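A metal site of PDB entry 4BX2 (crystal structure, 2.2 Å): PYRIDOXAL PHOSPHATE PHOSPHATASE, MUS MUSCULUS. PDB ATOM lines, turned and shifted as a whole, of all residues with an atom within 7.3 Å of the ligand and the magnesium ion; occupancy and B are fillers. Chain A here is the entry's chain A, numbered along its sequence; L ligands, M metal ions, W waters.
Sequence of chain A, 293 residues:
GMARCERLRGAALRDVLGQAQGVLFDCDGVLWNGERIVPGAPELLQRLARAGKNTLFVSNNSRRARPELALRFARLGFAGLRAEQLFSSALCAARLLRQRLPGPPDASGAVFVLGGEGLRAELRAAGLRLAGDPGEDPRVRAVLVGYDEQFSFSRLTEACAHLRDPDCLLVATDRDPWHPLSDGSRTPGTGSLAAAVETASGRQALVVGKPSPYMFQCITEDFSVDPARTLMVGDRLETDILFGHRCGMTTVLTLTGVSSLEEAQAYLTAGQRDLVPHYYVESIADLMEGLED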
ATOM      1  N   PHE A  25      21.035 -12.855  21.892  1.00  0.00           N
ATOM      2  CA  PHE A  25      20.026 -11.769  21.968  1.00  0.00           C
ATOM      3  C   PHE A  25      19.844 -11.310  23.397  1.00  0.00           C
ATOM      4  O   PHE A  25      19.633 -12.124  24.316  1.00  0.00           O
ATOM      5  CB  PHE A  25      18.656 -12.287  21.484  1.00  0.00           C
ATOM      6  CG  PHE A  25      18.535 -12.442  19.989  1.00  0.00           C
ATOM      7  CD1 PHE A  25      18.304 -11.341  19.165  1.00  0.00           C
ATOM      8  CD2 PHE A  25      18.636 -13.695  19.403  1.00  0.00           C
ATOM      9  CE1 PHE A  25      18.184 -11.491  17.786  1.00  0.00           C
ATOM     10  CE2 PHE A  25      18.478 -13.865  18.019  1.00  0.00           C
ATOM     11  CZ  PHE A  25      18.265 -12.753  17.205  1.00  0.00           C
ATOM     12  N   ASP A  26      19.988 -10.030  23.625  1.00  0.00           N
ATOM     13  CA  ASP A  26      19.444  -9.461  24.835  1.00  0.00           C
ATOM     14  C   ASP A  26      17.893  -9.583  24.681  1.00  0.00           C
ATOM     15  O   ASP A  26      17.373  -9.648  23.549  1.00  0.00           O
ATOM     16  CB  ASP A  26      19.887  -7.988  24.985  1.00  0.00           C
ATOM     17  CG  ASP A  26      19.066  -7.229  26.014  1.00  0.00           C
ATOM     18  OD1 ASP A  26      19.074  -7.607  27.197  1.00  0.00           O
ATOM     19  OD2 ASP A  26      18.316  -6.314  25.618  1.00  0.00           O
ATOM     20  N   CYS A  27      17.128  -9.541  25.773  1.00  0.00           N
ATOM     21  CA  CYS A  27      15.664  -9.761  25.647  1.00  0.00           C
ATOM     22  C   CYS A  27      14.793  -8.504  25.744  1.00  0.00           C
ATOM     23  O   CYS A  27      14.082  -8.152  24.782  1.00  0.00           O
ATOM     24  CB  CYS A  27      15.205 -10.789  26.673  1.00  0.00           C
ATOM     25  SG  CYS A  27      16.023 -12.390  26.507  1.00  0.00           S
ATOM     26  N   ASP A  28      14.825  -7.814  26.879  1.00  0.00           N
ATOM     27  CA  ASP A  28      14.000  -6.617  27.025  1.00  0.00           C
ATOM     28  C   ASP A  28      14.442  -5.510  26.086  1.00  0.00           C
ATOM     29  O   ASP A  28      15.615  -5.245  25.938  1.00  0.00           O
ATOM     30  CB  ASP A  28      13.989  -6.128  28.482  1.00  0.00           C
ATOM     31  CG  ASP A  28      13.564  -7.241  29.470  1.00  0.00           C
ATOM     32  OD1 ASP A  28      12.883  -8.192  29.023  1.00  0.00           O
ATOM     33  OD2 ASP A  28      13.900  -7.172  30.662  1.00  0.00           O
ATOM     34  N   GLY A  29      13.451  -4.862  25.461  1.00  0.00           N
ATOM     35  CA  GLY A  29      13.711  -3.816  24.496  1.00  0.00           C
ATOM     36  C   GLY A  29      14.125  -4.332  23.116  1.00  0.00           C
ATOM     37  O   GLY A  29      14.253  -3.535  22.187  1.00  0.00           O
ATOM     38  N   VAL A  30      14.277  -5.664  22.973  1.00  0.00           N
ATOM     39  CA  VAL A  30      14.792  -6.329  21.755  1.00  0.00           C
ATOM     40  C   VAL A  30      13.758  -7.336  21.153  1.00  0.00           C
ATOM     41  O   VAL A  30      13.421  -7.294  19.974  1.00  0.00           O
ATOM     42  CB  VAL A  30      16.093  -7.072  22.107  1.00  0.00           C
ATOM     43  CG1 VAL A  30      16.654  -7.880  20.938  1.00  0.00           C
ATOM     44  CG2 VAL A  30      17.175  -6.092  22.644  1.00  0.00           C
ATOM     45  N   LEU A  31      13.283  -8.266  21.984  1.00  0.00           N
ATOM     46  CA  LEU A  31      12.292  -9.226  21.524  1.00  0.00           C
ATOM     47  C   LEU A  31      10.900  -8.705  21.838  1.00  0.00           C
ATOM     48  O   LEU A  31       9.892  -9.116  21.239  1.00  0.00           O
ATOM     49  CB  LEU A  31      12.483 -10.558  22.241  1.00  0.00           C
ATOM     50  CG  LEU A  31      13.856 -11.213  22.119  1.00  0.00           C
ATOM     51  CD1 LEU A  31      13.890 -12.449  23.006  1.00  0.00           C
ATOM     52  CD2 LEU A  31      14.170 -11.577  20.692  1.00  0.00           C
ATOM     53  N   TRP A  32      10.850  -7.815  22.814  1.00  0.00           N
ATOM     54  CA  TRP A  32       9.592  -7.308  23.301  1.00  0.00           C
ATOM     55  C   TRP A  32       9.851  -6.023  24.098  1.00  0.00           C
ATOM     56  O   TRP A  32      10.974  -5.751  24.547  1.00  0.00           O
ATOM     57  CB  TRP A  32       8.938  -8.361  24.182  1.00  0.00           C
ATOM     58  CG  TRP A  32       9.770  -8.851  25.281  1.00  0.00           C
ATOM     59  CD1 TRP A  32      10.259  -8.117  26.319  1.00  0.00           C
ATOM     60  CD2 TRP A  32      10.200 -10.210  25.516  1.00  0.00           C
ATOM     61  NE1 TRP A  32      10.975  -8.907  27.172  1.00  0.00           N
ATOM     62  CE2 TRP A  32      10.972 -10.195  26.715  1.00  0.00           C
ATOM     63  CE3 TRP A  32      10.024 -11.416  24.836  1.00  0.00           C
ATOM     64  CZ2 TRP A  32      11.569 -11.361  27.245  1.00  0.00           C
ATOM     65  CZ3 TRP A  32      10.632 -12.576  25.354  1.00  0.00           C
ATOM     66  CH2 TRP A  32      11.404 -12.534  26.541  1.00  0.00           C
ATOM     67  N   VAL A  58      20.407 -13.510  26.632  1.00  0.00           N
ATOM     68  CA  VAL A  58      20.930 -12.946  27.872  1.00  0.00           C
ATOM     69  C   VAL A  58      20.011 -11.820  28.323  1.00  0.00           C
ATOM     70  O   VAL A  58      19.440 -11.128  27.511  1.00  0.00           O
ATOM     71  CB  VAL A  58      22.321 -12.364  27.742  1.00  0.00           C
ATOM     72  CG1 VAL A  58      23.304 -13.436  27.820  1.00  0.00           C
ATOM     73  CG2 VAL A  58      22.477 -11.512  26.423  1.00  0.00           C
ATOM     74  N   SER A  59      19.769 -11.721  29.609  1.00  0.00           N
ATOM     75  CA  SER A  59      18.990 -10.618  30.088  1.00  0.00           C
ATOM     76  C   SER A  59      19.507 -10.193  31.422  1.00  0.00           C
ATOM     77  O   SER A  59      19.880 -11.056  32.236  1.00  0.00           O
ATOM     78  CB  SER A  59      17.527 -11.020  30.196  1.00  0.00           C
ATOM     79  OG  SER A  59      16.845  -9.933  30.759  1.00  0.00           O
ATOM     80  N   ASN A  60      19.499  -8.882  31.697  1.00  0.00           N
ATOM     81  CA  ASN A  60      19.859  -8.461  33.054  1.00  0.00           C
ATOM     82  C   ASN A  60      18.661  -8.468  33.978  1.00  0.00           C
ATOM     83  O   ASN A  60      18.809  -8.222  35.180  1.00  0.00           O
ATOM     84  CB  ASN A  60      20.574  -7.114  33.082  1.00  0.00           C
ATOM     85  CG  ASN A  60      22.059  -7.241  32.751  1.00  0.00           C
ATOM     86  OD1 ASN A  60      22.628  -8.340  32.722  1.00  0.00           O
ATOM     87  ND2 ASN A  60      22.696  -6.101  32.455  1.00  0.00           N
ATOM     88  N   ASN A  61      17.492  -8.785  33.423  1.00  0.00           N
ATOM     89  CA  ASN A  61      16.255  -8.883  34.220  1.00  0.00           C
ATOM     90  C   ASN A  61      16.397  -9.998  35.267  1.00  0.00           C
ATOM     91  O   ASN A  61      16.608 -11.179  34.924  1.00  0.00           O
ATOM     92  CB  ASN A  61      15.058  -9.163  33.299  1.00  0.00           C
ATOM     93  CG  ASN A  61      13.740  -8.815  33.914  1.00  0.00           C
ATOM     94  OD1 ASN A  61      13.539  -9.050  35.100  1.00  0.00           O
ATOM     95  ND2 ASN A  61      12.821  -8.305  33.122  1.00  0.00           N
ATOM     96  N   ASP A 176      22.442  -2.046  35.668  1.00  0.00           N
ATOM     97  CA  ASP A 176      21.567  -1.244  34.835  1.00  0.00           C
ATOM     98  C   ASP A 176      20.957  -0.153  35.752  1.00  0.00           C
ATOM     99  O   ASP A 176      20.453  -0.454  36.840  1.00  0.00           O
ATOM    100  CB  ASP A 176      20.477  -2.086  34.209  1.00  0.00           C
ATOM    101  CG  ASP A 176      21.005  -3.049  33.136  1.00  0.00           C
ATOM    102  OD1 ASP A 176      22.197  -3.049  32.798  1.00  0.00           O
ATOM    103  OD2 ASP A 176      20.173  -3.752  32.563  1.00  0.00           O
ATOM    104  N   HIS A 179      15.034   1.499  34.216  1.00  0.00           N
ATOM    105  CA  HIS A 179      14.356   0.853  33.091  1.00  0.00           C
ATOM    106  C   HIS A 179      13.078   1.560  32.750  1.00  0.00           C
ATOM    107  O   HIS A 179      12.389   2.012  33.643  1.00  0.00           O
ATOM    108  CB  HIS A 179      14.034  -0.605  33.465  1.00  0.00           C
ATOM    109  CG  HIS A 179      15.235  -1.369  33.892  1.00  0.00           C
ATOM    110  ND1 HIS A 179      16.100  -1.959  32.988  1.00  0.00           N
ATOM    111  CD2 HIS A 179      15.775  -1.563  35.113  1.00  0.00           C
ATOM    112  CE1 HIS A 179      17.098  -2.518  33.637  1.00  0.00           C
ATOM    113  NE2 HIS A 179      16.928  -2.310  34.932  1.00  0.00           N
ATOM    114  N   LYS A 210      25.813  -8.546  32.207  1.00  0.00           N
ATOM    115  CA  LYS A 210      26.369  -7.677  31.169  1.00  0.00           C
ATOM    116  C   LYS A 210      26.425  -6.268  31.738  1.00  0.00           C
ATOM    117  O   LYS A 210      25.418  -5.779  32.250  1.00  0.00           O
ATOM    118  CB  LYS A 210      25.380  -7.545  30.000  1.00  0.00           C
ATOM    119  CG  LYS A 210      24.908  -8.731  29.292  1.00  0.00           C
ATOM    120  CD  LYS A 210      23.732  -8.329  28.390  1.00  0.00           C
ATOM    121  CE  LYS A 210      22.512  -8.139  29.177  1.00  0.00           C
ATOM    122  NZ  LYS A 210      21.408  -7.436  28.503  1.00  0.00           N
ATOM    123  N   MET A 215      29.047 -12.984  32.686  1.00  0.00           N
ATOM    124  CA  MET A 215      27.893 -13.469  31.961  1.00  0.00           C
ATOM    125  C   MET A 215      28.331 -14.283  30.778  1.00  0.00           C
ATOM    126  O   MET A 215      27.713 -15.289  30.457  1.00  0.00           O
ATOM    127  CB  MET A 215      26.992 -12.324  31.503  1.00  0.00           C
ATOM    128  CG  MET A 215      25.610 -12.800  31.156  1.00  0.00           C
ATOM    129  SD  MET A 215      24.381 -11.436  31.020  1.00  0.00           S
ATOM    130  CE  MET A 215      23.410 -11.967  32.452  1.00  0.00           C
ATOM    131  N   VAL A 233      23.315  -8.875  20.020  1.00  0.00           N
ATOM    132  CA  VAL A 233      22.248  -7.977  19.612  1.00  0.00           C
ATOM    133  C   VAL A 233      21.571  -7.408  20.849  1.00  0.00           C
ATOM    134  O   VAL A 233      21.050  -8.157  21.671  1.00  0.00           O
ATOM    135  CB  VAL A 233      21.190  -8.683  18.767  1.00  0.00           C
ATOM    136  CG1 VAL A 233      20.043  -7.713  18.431  1.00  0.00           C
ATOM    137  CG2 VAL A 233      21.764  -9.277  17.523  1.00  0.00           C
ATOM    138  N   GLY A 234      21.538  -6.091  20.964  1.00  0.00           N
ATOM    139  CA  GLY A 234      20.963  -5.448  22.126  1.00  0.00           C
ATOM    140  C   GLY A 234      20.403  -4.061  21.872  1.00  0.00           C
ATOM    141  O   GLY A 234      20.628  -3.472  20.829  1.00  0.00           O
ATOM    142  N   ASP A 235      19.626  -3.543  22.815  1.00  0.00           N
ATOM    143  CA  ASP A 235      19.089  -2.201  22.683  1.00  0.00           C
ATOM    144  C   ASP A 235      19.831  -1.173  23.566  1.00  0.00           C
ATOM    145  O   ASP A 235      19.535   0.020  23.520  1.00  0.00           O
ATOM    146  CB  ASP A 235      17.611  -2.209  23.079  1.00  0.00           C
ATOM    147  CG  ASP A 235      17.411  -2.587  24.515  1.00  0.00           C
ATOM    148  OD1 ASP A 235      17.872  -3.697  24.902  1.00  0.00           O
ATOM    149  OD2 ASP A 235      16.820  -1.762  25.242  1.00  0.00           O
ATOM    150  N   ARG A 236      20.762  -1.626  24.389  1.00  0.00           N
ATOM    151  CA  ARG A 236      21.383  -0.694  25.347  1.00  0.00           C
ATOM    152  C   ARG A 236      22.892  -0.592  25.163  1.00  0.00           C
ATOM    153  O   ARG A 236      23.642  -1.549  25.367  1.00  0.00           O
ATOM    154  CB  ARG A 236      21.006  -1.083  26.764  1.00  0.00           C
ATOM    155  CG  ARG A 236      21.178   0.005  27.821  1.00  0.00           C
ATOM    156  CD  ARG A 236      20.268  -0.279  29.024  1.00  0.00           C
ATOM    157  NE  ARG A 236      20.128   0.909  29.896  1.00  0.00           N
ATOM    158  CZ  ARG A 236      19.227   1.033  30.856  1.00  0.00           C
ATOM    159  NH1 ARG A 236      18.363   0.056  31.089  1.00  0.00           N
ATOM    160  NH2 ARG A 236      19.177   2.159  31.576  1.00  0.00           N
ATOM    161  N   THR A 239      25.267  -1.352  28.221  1.00  0.00           N
ATOM    162  CA  THR A 239      25.276  -2.701  28.701  1.00  0.00           C
ATOM    163  C   THR A 239      25.501  -3.747  27.592  1.00  0.00           C
ATOM    164  O   THR A 239      26.399  -4.547  27.703  1.00  0.00           O
ATOM    165  CB  THR A 239      23.998  -3.065  29.514  1.00  0.00           C
ATOM    166  OG1 THR A 239      22.956  -3.425  28.628  1.00  0.00           O
ATOM    167  CG2 THR A 239      23.529  -1.937  30.371  1.00  0.00           C
ATOM    168  N   ASP A 240      24.667  -3.770  26.563  1.00  0.00           N
ATOM    169  CA  ASP A 240      24.737  -4.811  25.526  1.00  0.00           C
ATOM    170  C   ASP A 240      25.918  -4.652  24.604  1.00  0.00           C
ATOM    171  O   ASP A 240      26.655  -5.619  24.337  1.00  0.00           O
ATOM    172  CB  ASP A 240      23.414  -4.830  24.742  1.00  0.00           C
ATOM    173  CG  ASP A 240      22.230  -4.961  25.689  1.00  0.00           C
ATOM    174  OD1 ASP A 240      22.386  -5.765  26.634  1.00  0.00           O
ATOM    175  OD2 ASP A 240      21.199  -4.280  25.542  1.00  0.00           O
ATOM    176  N   THR A 254      19.855  -2.588  18.171  1.00  0.00           N
ATOM    177  CA  THR A 254      18.492  -2.448  17.654  1.00  0.00           C
ATOM    178  C   THR A 254      17.840  -1.247  18.346  1.00  0.00           C
ATOM    179  O   THR A 254      18.112  -0.978  19.522  1.00  0.00           O
ATOM    180  CB  THR A 254      17.667  -3.738  17.900  1.00  0.00           C
ATOM    181  OG1 THR A 254      16.325  -3.538  17.401  1.00  0.00           O
ATOM    182  CG2 THR A 254      17.609  -4.032  19.363  1.00  0.00           C
ATOM    183  N   GLY A 257      14.353  -0.146  21.605  1.00  0.00           N
ATOM    184  CA  GLY A 257      14.499  -0.148  23.035  1.00  0.00           C
ATOM    185  C   GLY A 257      15.092   1.110  23.635  1.00  0.00           C
ATOM    186  O   GLY A 257      14.734   2.204  23.260  1.00  0.00           O
ATOM    187  N   VAL A 258      16.011   0.947  24.588  1.00  0.00           N
ATOM    188  CA  VAL A 258      16.443   2.081  25.404  1.00  0.00           C
ATOM    189  C   VAL A 258      17.324   3.105  24.654  1.00  0.00           C
ATOM    190  O   VAL A 258      17.027   4.263  24.709  1.00  0.00           O
ATOM    191  CB  VAL A 258      17.183   1.598  26.679  1.00  0.00           C
ATOM    192  CG1 VAL A 258      17.749   2.799  27.473  1.00  0.00           C
ATOM    193  CG2 VAL A 258      16.243   0.758  27.564  1.00  0.00           C
HETATM  194 BE1  LIG L   1      17.995  -7.201  28.299  1.00  0.00          BE
HETATM  195  F1  LIG L   1      17.299  -5.817  28.153  1.00  0.00           F
HETATM  196  F2  LIG L   1      18.840  -7.246  29.583  1.00  0.00           F
HETATM  197  F3  LIG L   1      16.925  -8.282  28.485  1.00  0.00           F
HETATM  198 MG    MG M   1      17.481  -4.712  26.610  1.00  0.00          MG
HETATM  199  O   HOH W   1      16.681  -3.025  27.692  1.00  0.00           O
HETATM  200  O   HOH W   2      19.351  -4.182  27.473  1.00  0.00           O
HETATM  201  O   HOH W   3      20.196  -4.139  30.051  1.00  0.00           O
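Water W3 lies within hydrogen-bond range of OD2 of Asp 176 (2.5 Å), OG1 of Thr 239 (3.2 Å) and F2 of the ligand (3.4 Å).
Residues that only touch the magnesium ion: Asp 240. Within 4 Å of the magnesium ion: Asp 26, Asp 28, Asp 235 and Asp 240. The nearest printed residue that does not touch the magnesium ion is Gly 29 (4.2 Å).
NZ of Lys 210 sits close to OD1 of Asp 26 (2.7 Å). The backbone NH (N) of Asp 235 is in hydrogen-bond range of the side-chain carboxylate (OD2) of Asp 240, at 3.2 Å. The side-chain amide nitrogen (ND2) of Asn 61 is in hydrogen-bond range of the side-chain carboxylate (OD2) of Asp 28 (2.9 Å). The indole nitrogen (NE1) of Trp 32 lies within hydrogen-bond range of the side-chain carboxylate (OD1) of Asp 28 (2.8 Å). The side-chain amide nitrogen of Asn 60 lies within hydrogen-bond range of the backbone carbonyl oxygen of Lys 210 (2.7 Å). The side-chain carboxylate of Asp 240 lies within salt-bridge range of the side-chain amino group of Lys 210 (2.7 Å). N of Lys 210 sits close to SD of Met 215 (3.4 Å). O of Phe 25 lies within hydrogen-bond range of N of Val 58.
Residues that only touch the ligand: Val 58 (3.9 Å). Eight residues have an atom within 4 Å of the ligand: Asp 26, Cys 27, Asp 28, Val 58, Ser 59, Asn 60, Lys 210 and Asp 235. Along chain A the residues within 4 Å of the ligand span positions 26 to 235.
The magnesium ion is bound by a fluorine (F1) of the ligand (1.9 Å), the side-chain carboxylate of Asp 235 (2.0 Å), the backbone carbonyl oxygen of Asp 28 (2.1 Å), the side-chain carboxylate of Asp 26 (2.1 Å), water W2 (2.1 Å) and water W1 (2.2 Å).
The side-chain carboxylate (OD1) of Asp 26 binds a beryllium atom (BE1) of the ligand (1.6 Å). The backbone NH (N) of Asp 28 sits at hydrogen-bond distance from a fluorine (F3) of the ligand (2.7 Å). A fluorine (F2) of the ligand lies within hydrogen-bond range of the backbone NH of Asn 60 (2.8 Å). The side-chain amino group (NZ) of Lys 210 is in hydrogen-bond range of a fluorine (F2) of the ligand (2.8 Å). The side-chain hydroxyl (OG) of Ser 59 lies within hydrogen-bond range of a fluorine (F3) of the ligand, at 2.8 Å. F3 of the ligand sits at hydrogen-bond distance from N of Cys 27, 3.0 Å away.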
